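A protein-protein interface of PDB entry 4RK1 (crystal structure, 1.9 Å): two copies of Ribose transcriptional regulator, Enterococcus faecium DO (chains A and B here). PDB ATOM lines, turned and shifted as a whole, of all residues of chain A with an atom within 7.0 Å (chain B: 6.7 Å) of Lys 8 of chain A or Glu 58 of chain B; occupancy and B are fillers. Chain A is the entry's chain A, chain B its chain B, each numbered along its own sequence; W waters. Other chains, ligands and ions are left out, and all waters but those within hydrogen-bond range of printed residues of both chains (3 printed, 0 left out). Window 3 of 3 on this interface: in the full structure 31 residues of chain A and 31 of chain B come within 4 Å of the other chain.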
ATOM      1  N   LYS A   8      -9.492  23.635  -4.157  1.00  0.00           N
ATOM      2  CA  LYS A   8     -10.054  22.252  -4.083  1.00  0.00           C
ATOM      3  C   LYS A   8     -11.547  22.173  -3.686  1.00  0.00           C
ATOM      4  O   LYS A   8     -12.063  21.084  -3.422  1.00  0.00           O
ATOM      5  CB  LYS A   8      -9.200  21.397  -3.132  1.00  0.00           C
ATOM      6  CG  LYS A   8      -7.929  20.834  -3.752  1.00  0.00           C
ATOM      7  CD  LYS A   8      -8.249  20.009  -4.989  1.00  0.00           C
ATOM      8  CE  LYS A   8      -7.065  19.191  -5.462  1.00  0.00           C
ATOM      9  NZ  LYS A   8      -7.233  18.862  -6.904  1.00  0.00           N
ATOM     10  N   THR A   9     -12.242  23.309  -3.670  1.00  0.00           N
ATOM     11  CA  THR A   9     -13.675  23.342  -3.355  1.00  0.00           C
ATOM     12  C   THR A   9     -14.418  23.979  -4.524  1.00  0.00           C
ATOM     13  O   THR A   9     -14.020  25.035  -5.024  1.00  0.00           O
ATOM     14  CB  THR A   9     -13.987  24.125  -2.050  1.00  0.00           C
ATOM     15  OG1 THR A   9     -13.320  23.521  -0.936  1.00  0.00           O
ATOM     16  CG2 THR A   9     -15.475  24.102  -1.749  1.00  0.00           C
ATOM     17  N   ILE A  10     -15.496  23.326  -4.952  1.00  0.00           N
ATOM     18  CA  ILE A  10     -16.351  23.824  -6.017  1.00  0.00           C
ATOM     19  C   ILE A  10     -17.730  24.091  -5.436  1.00  0.00           C
ATOM     20  O   ILE A  10     -18.259  23.263  -4.705  1.00  0.00           O
ATOM     21  CB  ILE A  10     -16.474  22.785  -7.151  1.00  0.00           C
ATOM     22  CG1 ILE A  10     -15.105  22.504  -7.791  1.00  0.00           C
ATOM     23  CG2 ILE A  10     -17.472  23.247  -8.201  1.00  0.00           C
ATOM     24  CD1 ILE A  10     -14.425  23.720  -8.372  1.00  0.00           C
ATOM     25  N   GLN A  36     -11.340  13.801  -8.905  1.00  0.00           N
ATOM     26  CA  GLN A  36     -10.192  14.714  -8.924  1.00  0.00           C
ATOM     27  C   GLN A  36      -9.939  15.346  -7.562  1.00  0.00           C
ATOM     28  O   GLN A  36      -9.323  16.406  -7.477  1.00  0.00           O
ATOM     29  CB  GLN A  36     -10.399  15.803  -9.981  1.00  0.00           C
ATOM     30  CG  GLN A  36     -10.665  15.266 -11.378  1.00  0.00           C
ATOM     31  CD  GLN A  36      -9.542  14.392 -11.902  1.00  0.00           C
ATOM     32  OE1 GLN A  36      -8.365  14.705 -11.727  1.00  0.00           O
ATOM     33  NE2 GLN A  36      -9.902  13.289 -12.552  1.00  0.00           N
ATOM     34  N   ASN A  37     -10.418  14.687  -6.505  1.00  0.00           N
ATOM     35  CA  ASN A  37     -10.254  15.139  -5.120  1.00  0.00           C
ATOM     36  C   ASN A  37     -10.774  16.545  -4.840  1.00  0.00           C
ATOM     37  O   ASN A  37     -10.228  17.253  -3.996  1.00  0.00           O
ATOM     38  CB  ASN A  37      -8.787  15.013  -4.675  1.00  0.00           C
ATOM     39  CG  ASN A  37      -8.266  13.590  -4.779  1.00  0.00           C
ATOM     40  OD1 ASN A  37      -9.000  12.630  -4.548  1.00  0.00           O
ATOM     41  ND2 ASN A  37      -6.992  13.450  -5.127  1.00  0.00           N
ATOM     42  N   PHE A  38     -11.837  16.942  -5.536  1.00  0.00           N
ATOM     43  CA  PHE A  38     -12.517  18.188  -5.222  1.00  0.00           C
ATOM     44  C   PHE A  38     -13.629  17.930  -4.221  1.00  0.00           C
ATOM     45  O   PHE A  38     -14.271  16.882  -4.239  1.00  0.00           O
ATOM     46  CB  PHE A  38     -13.106  18.837  -6.476  1.00  0.00           C
ATOM     47  CG  PHE A  38     -12.111  19.611  -7.281  1.00  0.00           C
ATOM     48  CD1 PHE A  38     -11.891  20.959  -7.030  1.00  0.00           C
ATOM     49  CD2 PHE A  38     -11.390  18.991  -8.288  1.00  0.00           C
ATOM     50  CE1 PHE A  38     -10.971  21.676  -7.775  1.00  0.00           C
ATOM     51  CE2 PHE A  38     -10.467  19.703  -9.038  1.00  0.00           C
ATOM     52  CZ  PHE A  38     -10.260  21.047  -8.783  1.00  0.00           C
ATOM     53  N   VAL A  39     -13.839  18.903  -3.347  1.00  0.00           N
ATOM     54  CA  VAL A  39     -14.970  18.915  -2.448  1.00  0.00           C
ATOM     55  C   VAL A  39     -16.062  19.709  -3.135  1.00  0.00           C
ATOM     56  O   VAL A  39     -15.805  20.805  -3.639  1.00  0.00           O
ATOM     57  CB  VAL A  39     -14.596  19.561  -1.090  1.00  0.00           C
ATOM     58  CG1 VAL A  39     -15.824  19.751  -0.214  1.00  0.00           C
ATOM     59  CG2 VAL A  39     -13.564  18.701  -0.374  1.00  0.00           C
ATOM     60  N   THR A  40     -17.261  19.134  -3.179  1.00  0.00           N
ATOM     61  CA  THR A  40     -18.426  19.791  -3.750  1.00  0.00           C
ATOM     62  C   THR A  40     -19.354  20.282  -2.652  1.00  0.00           C
ATOM     63  O   THR A  40     -19.777  19.512  -1.784  1.00  0.00           O
ATOM     64  CB  THR A  40     -19.221  18.837  -4.660  1.00  0.00           C
ATOM     65  OG1 THR A  40     -18.326  18.158  -5.550  1.00  0.00           O
ATOM     66  CG2 THR A  40     -20.268  19.619  -5.470  1.00  0.00           C
ATOM     67  N   ARG A  62     -14.297  32.892   0.914  1.00  0.00           N
ATOM     68  CA  ARG A  62     -13.900  31.614   1.501  1.00  0.00           C
ATOM     69  C   ARG A  62     -12.943  30.826   0.592  1.00  0.00           C
ATOM     70  O   ARG A  62     -12.517  29.730   0.955  1.00  0.00           O
ATOM     71  CB  ARG A  62     -15.132  30.747   1.835  1.00  0.00           C
ATOM     72  CG  ARG A  62     -16.205  31.393   2.723  1.00  0.00           C
ATOM     73  CD  ARG A  62     -15.923  31.246   4.209  1.00  0.00           C
ATOM     74  NE  ARG A  62     -14.685  31.929   4.571  1.00  0.00           N
ATOM     75  CZ  ARG A  62     -14.573  33.234   4.822  1.00  0.00           C
ATOM     76  NH1 ARG A  62     -13.383  33.740   5.137  1.00  0.00           N
ATOM     77  NH2 ARG A  62     -15.634  34.035   4.773  1.00  0.00           N
ATOM     78  N   GLY A  63     -12.588  31.367  -0.576  1.00  0.00           N
ATOM     79  CA  GLY A  63     -11.630  30.702  -1.454  1.00  0.00           C
ATOM     80  C   GLY A  63     -12.207  29.558  -2.283  1.00  0.00           C
ATOM     81  O   GLY A  63     -11.466  28.720  -2.785  1.00  0.00           O
ATOM     82  N   VAL A  64     -13.524  29.532  -2.456  1.00  0.00           N
ATOM     83  CA  VAL A  64     -14.145  28.559  -3.359  1.00  0.00           C
ATOM     84  C   VAL A  64     -13.523  28.766  -4.744  1.00  0.00           C
ATOM     85  O   VAL A  64     -13.463  29.879  -5.262  1.00  0.00           O
ATOM     86  CB  VAL A  64     -15.681  28.673  -3.356  1.00  0.00           C
ATOM     87  CG1 VAL A  64     -16.302  27.795  -4.429  1.00  0.00           C
ATOM     88  CG2 VAL A  64     -16.226  28.281  -1.991  1.00  0.00           C
ATOM     89  N   ASP A  65     -13.059  27.674  -5.333  1.00  0.00           N
ATOM     90  CA  ASP A  65     -12.185  27.777  -6.483  1.00  0.00           C
ATOM     91  C   ASP A  65     -12.933  27.948  -7.815  1.00  0.00           C
ATOM     92  O   ASP A  65     -12.412  28.568  -8.735  1.00  0.00           O
ATOM     93  CB  ASP A  65     -11.209  26.605  -6.467  1.00  0.00           C
ATOM     94  CG  ASP A  65     -10.328  26.614  -5.211  1.00  0.00           C
ATOM     95  OD1 ASP A  65     -10.754  26.093  -4.144  1.00  0.00           O
ATOM     96  OD2 ASP A  65      -9.219  27.187  -5.283  1.00  0.00           O
ATOM     97  N   ILE B  53     -12.732  11.421   1.088  1.00  0.00           N
ATOM     98  CA  ILE B  53     -12.139  12.746   0.916  1.00  0.00           C
ATOM     99  C   ILE B  53     -12.357  13.581   2.190  1.00  0.00           C
ATOM    100  O   ILE B  53     -13.392  13.470   2.851  1.00  0.00           O
ATOM    101  CB  ILE B  53     -12.697  13.445  -0.361  1.00  0.00           C
ATOM    102  CG1 ILE B  53     -11.573  14.112  -1.178  1.00  0.00           C
ATOM    103  CG2 ILE B  53     -13.846  14.405  -0.047  1.00  0.00           C
ATOM    104  CD1 ILE B  53     -10.811  15.230  -0.489  1.00  0.00           C
ATOM    105  N   GLU B  54     -11.361  14.396   2.530  1.00  0.00           N
ATOM    106  CA  GLU B  54     -11.382  15.241   3.728  1.00  0.00           C
ATOM    107  C   GLU B  54     -12.283  16.481   3.620  1.00  0.00           C
ATOM    108  O   GLU B  54     -11.811  17.592   3.381  1.00  0.00           O
ATOM    109  CB  GLU B  54      -9.950  15.668   4.061  1.00  0.00           C
ATOM    110  CG  GLU B  54      -9.045  14.502   4.445  1.00  0.00           C
ATOM    111  CD  GLU B  54      -7.594  14.713   4.060  1.00  0.00           C
ATOM    112  OE1 GLU B  54      -7.277  15.723   3.393  1.00  0.00           O
ATOM    113  OE2 GLU B  54      -6.761  13.857   4.421  1.00  0.00           O
ATOM    114  N   TYR B  55     -13.580  16.278   3.836  1.00  0.00           N
ATOM    115  CA  TYR B  55     -14.552  17.377   3.846  1.00  0.00           C
ATOM    116  C   TYR B  55     -14.197  18.427   4.892  1.00  0.00           C
ATOM    117  O   TYR B  55     -14.044  19.604   4.573  1.00  0.00           O
ATOM    118  CB  TYR B  55     -15.969  16.850   4.112  1.00  0.00           C
ATOM    119  CG  TYR B  55     -16.534  16.022   2.978  1.00  0.00           C
ATOM    120  CD1 TYR B  55     -17.215  16.624   1.925  1.00  0.00           C
ATOM    121  CD2 TYR B  55     -16.387  14.634   2.958  1.00  0.00           C
ATOM    122  CE1 TYR B  55     -17.734  15.872   0.883  1.00  0.00           C
ATOM    123  CE2 TYR B  55     -16.902  13.873   1.921  1.00  0.00           C
ATOM    124  CZ  TYR B  55     -17.574  14.495   0.885  1.00  0.00           C
ATOM    125  OH  TYR B  55     -18.083  13.742  -0.146  1.00  0.00           O
ATOM    126  N   LEU B  56     -14.050  17.997   6.142  1.00  0.00           N
ATOM    127  CA  LEU B  56     -13.824  18.933   7.246  1.00  0.00           C
ATOM    128  C   LEU B  56     -12.549  19.731   7.097  1.00  0.00           C
ATOM    129  O   LEU B  56     -12.545  20.949   7.323  1.00  0.00           O
ATOM    130  CB  LEU B  56     -13.794  18.205   8.590  1.00  0.00           C
ATOM    131  CG  LEU B  56     -15.104  17.693   9.168  1.00  0.00           C
ATOM    132  CD1 LEU B  56     -14.845  17.184  10.579  1.00  0.00           C
ATOM    133  CD2 LEU B  56     -16.182  18.770   9.155  1.00  0.00           C
ATOM    134  N   ALA B  57     -11.466  19.049   6.729  1.00  0.00           N
ATOM    135  CA  ALA B  57     -10.167  19.698   6.590  1.00  0.00           C
ATOM    136  C   ALA B  57     -10.240  20.795   5.536  1.00  0.00           C
ATOM    137  O   ALA B  57      -9.832  21.929   5.775  1.00  0.00           O
ATOM    138  CB  ALA B  57      -9.087  18.679   6.228  1.00  0.00           C
ATOM    139  N   GLU B  58     -10.781  20.461   4.372  1.00  0.00           N
ATOM    140  CA  GLU B  58     -10.902  21.437   3.301  1.00  0.00           C
ATOM    141  C   GLU B  58     -11.823  22.592   3.718  1.00  0.00           C
ATOM    142  O   GLU B  58     -11.479  23.750   3.537  1.00  0.00           O
ATOM    143  CB  GLU B  58     -11.408  20.756   2.022  1.00  0.00           C
ATOM    144  CG  GLU B  58     -11.668  21.684   0.842  1.00  0.00           C
ATOM    145  CD  GLU B  58     -10.441  22.461   0.371  1.00  0.00           C
ATOM    146  OE1 GLU B  58      -9.296  22.016   0.612  1.00  0.00           O
ATOM    147  OE2 GLU B  58     -10.628  23.528  -0.254  1.00  0.00           O
ATOM    148  N   LEU B  59     -12.992  22.277   4.261  1.00  0.00           N
ATOM    149  CA  LEU B  59     -13.955  23.316   4.632  1.00  0.00           C
ATOM    150  C   LEU B  59     -13.438  24.205   5.763  1.00  0.00           C
ATOM    151  O   LEU B  59     -13.664  25.414   5.760  1.00  0.00           O
ATOM    152  CB  LEU B  59     -15.299  22.685   5.001  1.00  0.00           C
ATOM    153  CG  LEU B  59     -16.085  22.065   3.832  1.00  0.00           C
ATOM    154  CD1 LEU B  59     -17.462  21.627   4.299  1.00  0.00           C
ATOM    155  CD2 LEU B  59     -16.206  23.041   2.675  1.00  0.00           C
ATOM    156  N   THR B  60     -12.725  23.603   6.712  1.00  0.00           N
ATOM    157  CA  THR B  60     -12.062  24.352   7.773  1.00  0.00           C
ATOM    158  C   THR B  60     -11.039  25.326   7.198  1.00  0.00           C
ATOM    159  O   THR B  60     -11.035  26.494   7.579  1.00  0.00           O
ATOM    160  CB  THR B  60     -11.418  23.396   8.801  1.00  0.00           C
ATOM    161  OG1 THR B  60     -12.441  22.565   9.364  1.00  0.00           O
ATOM    162  CG2 THR B  60     -10.729  24.164   9.933  1.00  0.00           C
ATOM    163  N   ARG B  61     -10.217  24.860   6.252  1.00  0.00           N
ATOM    164  CA  ARG B  61      -9.257  25.733   5.555  1.00  0.00           C
ATOM    165  C   ARG B  61      -9.953  26.867   4.813  1.00  0.00           C
ATOM    166  O   ARG B  61      -9.423  27.968   4.738  1.00  0.00           O
ATOM    167  CB  ARG B  61      -8.380  24.947   4.575  1.00  0.00           C
ATOM    168  CG  ARG B  61      -7.253  24.157   5.234  1.00  0.00           C
ATOM    169  CD  ARG B  61      -6.228  23.697   4.209  1.00  0.00           C
ATOM    170  NE  ARG B  61      -6.808  22.736   3.274  1.00  0.00           N
ATOM    171  CZ  ARG B  61      -6.776  21.410   3.410  1.00  0.00           C
ATOM    172  NH1 ARG B  61      -6.174  20.837   4.449  1.00  0.00           N
ATOM    173  NH2 ARG B  61      -7.356  20.644   2.488  1.00  0.00           N
ATOM    174  N   ARG B  62     -11.147  26.606   4.293  1.00  0.00           N
ATOM    175  CA  ARG B  62     -11.922  27.643   3.608  1.00  0.00           C
ATOM    176  C   ARG B  62     -12.557  28.645   4.591  1.00  0.00           C
ATOM    177  O   ARG B  62     -13.262  29.551   4.167  1.00  0.00           O
ATOM    178  CB  ARG B  62     -13.013  27.013   2.720  1.00  0.00           C
ATOM    179  CG  ARG B  62     -12.538  26.017   1.656  1.00  0.00           C
ATOM    180  CD  ARG B  62     -12.055  26.669   0.365  1.00  0.00           C
ATOM    181  NE  ARG B  62     -10.902  27.534   0.600  1.00  0.00           N
ATOM    182  CZ  ARG B  62      -9.651  27.115   0.807  1.00  0.00           C
ATOM    183  NH1 ARG B  62      -8.683  28.003   1.012  1.00  0.00           N
ATOM    184  NH2 ARG B  62      -9.352  25.824   0.811  1.00  0.00           N
ATOM    185  N   GLY B  63     -12.328  28.484   5.897  1.00  0.00           N
ATOM    186  CA  GLY B  63     -12.840  29.435   6.883  1.00  0.00           C
ATOM    187  C   GLY B  63     -14.307  29.258   7.243  1.00  0.00           C
ATOM    188  O   GLY B  63     -14.939  30.192   7.722  1.00  0.00           O
ATOM    189  N   VAL B  64     -14.858  28.066   7.016  1.00  0.00           N
ATOM    190  CA  VAL B  64     -16.240  27.789   7.419  1.00  0.00           C
ATOM    191  C   VAL B  64     -16.330  27.954   8.947  1.00  0.00           C
ATOM    192  O   VAL B  64     -15.515  27.419   9.684  1.00  0.00           O
ATOM    193  CB  VAL B  64     -16.711  26.410   6.923  1.00  0.00           C
ATOM    194  CG1 VAL B  64     -18.075  26.061   7.489  1.00  0.00           C
ATOM    195  CG2 VAL B  64     -16.754  26.400   5.395  1.00  0.00           C
ATOM    196  N   ASN B  82      -9.558  19.222  13.059  1.00  0.00           N
ATOM    197  CA  ASN B  82      -9.950  20.384  12.278  1.00  0.00           C
ATOM    198  C   ASN B  82     -10.843  21.360  13.033  1.00  0.00           C
ATOM    199  O   ASN B  82     -10.514  22.542  13.158  1.00  0.00           O
ATOM    200  CB  ASN B  82     -10.609  19.907  10.987  1.00  0.00           C
ATOM    201  CG  ASN B  82      -9.649  19.108  10.115  1.00  0.00           C
ATOM    202  OD1 ASN B  82      -8.706  19.665   9.559  1.00  0.00           O
ATOM    203  ND2 ASN B  82      -9.871  17.807  10.007  1.00  0.00           N
HETATM  204  O   HOH W   1     -11.017  31.874   5.112  1.00  0.00           O
HETATM  205  O   HOH W   2     -17.936  16.210  -2.152  1.00  0.00           O
HETATM  206  O   HOH W   3      -9.291  30.603   1.427  1.00  0.00           O
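OG1 of Thr 9 of chain A is in hydrogen-bond range of OE2 of Glu 58 of chain B (2.8 Å). O of Arg 62 of chain A lies within hydrogen-bond range of NE of Arg 62 of chain B (2.7 Å).
OE1 of Glu 58 of chain B lies within salt-bridge range of NH2 of Arg 61 of chain B (3.0 Å). N of Ile 10 of chain A is in hydrogen-bond range of O of Val 39 of chain A (2.9 Å). The backbone carbonyl oxygen of Lys 8 of chain A is in hydrogen-bond range of the backbone NH of Val 39 of chain A, at 2.8 Å. N of Asp 65 of chain A lies within hydrogen-bond range of O of Thr 9 of chain A, at 2.8 Å. NZ of Lys 8 of chain A is in hydrogen-bond range of O of Gln 36 of chain A, at 3.3 Å. The side-chain carboxylate (OE2) of Glu 58 of chain B is in salt-bridge range of the guanidinium group (NH2) of Arg 62 of chain B (2.8 Å).
Among the printed residues, merely in contact across the chains: Lys 8 of chain A with Glu 58 of chain B (3.8 Å), Thr 9 of chain A with Arg 62 of chain B (3.6 Å), Val 39 of chain A with Glu 58 of chain B (3.7 Å), Arg 62 of chain A with Gly 63 of chain B (3.6 Å) and Gly 63 of chain A with Arg 62 of chain B (3.6 Å).
Lys 8 of chain A touches just one residue of chain B: Glu 58. Of chain A, only Lys 8, Thr 9 and Val 39 come within 4 Å of Glu 58 of chain B. Printed residues of chain A within 4 Å of Gly 63 of chain B: Arg 62 (3.6 Å). Of the printed residues of chain B, Thr 9 of chain A touches Glu 58 and Arg 62. Thr 60 of chain B touches none of the printed residues of chain A. The nearest printed residue of chain A that does not touch Glu 58 of chain B is Asp 65 of chain A (4.7 Å). The nearest printed residue of chain B that does not touch Gly 63 of chain A is Glu 58 of chain B (5.8 Å).
Of the 13 printed residues of chain B, 3 touch a printed residue of chain A. Printed residues of chain B that touch a printed residue of chain A: Glu 58, Arg 62 and Gly 63. Of the 12 printed residues of chain A, 5 touch a printed residue of chain B. Hydrophobic or aromatic side chains of chain A that line the printed part of chain B: Val 39. Among the printed residues, 7 pairs touch across the chains. Among the printed residues, no Asp or Glu carboxylate lies within 4 Å of a Lys or Arg side-chain nitrogen of the other chain.
Arg 62 of chain A touches its own counterpart, Arg 62 of chain B. Arg 62 of chain A touches Gly 63 of chain B, and with the chains exchanged Gly 63 of chain A touches Arg 62 of chain B. Of the 7 pairs that touch across the chains among the printed residues, 3 have their exchanged pair printed and touching as well.
Water W3 bridges the guanidinium group of Arg 62 of chain B (2.7 Å) and the backbone carbonyl oxygen of Arg 62 of chain A (3.4 Å). Water W1 lies within hydrogen-bond range of the guanidinium group of Arg 62 of chain A (3.0 Å) and the backbone carbonyl oxygen of Arg 62 of chain B (3.4 Å). Water W2 lies within hydrogen-bond range of the backbone NH (N) of Thr 40 of chain A (3.2 Å) and the side-chain hydroxyl (OH) of Tyr 55 of chain B (3.2 Å).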
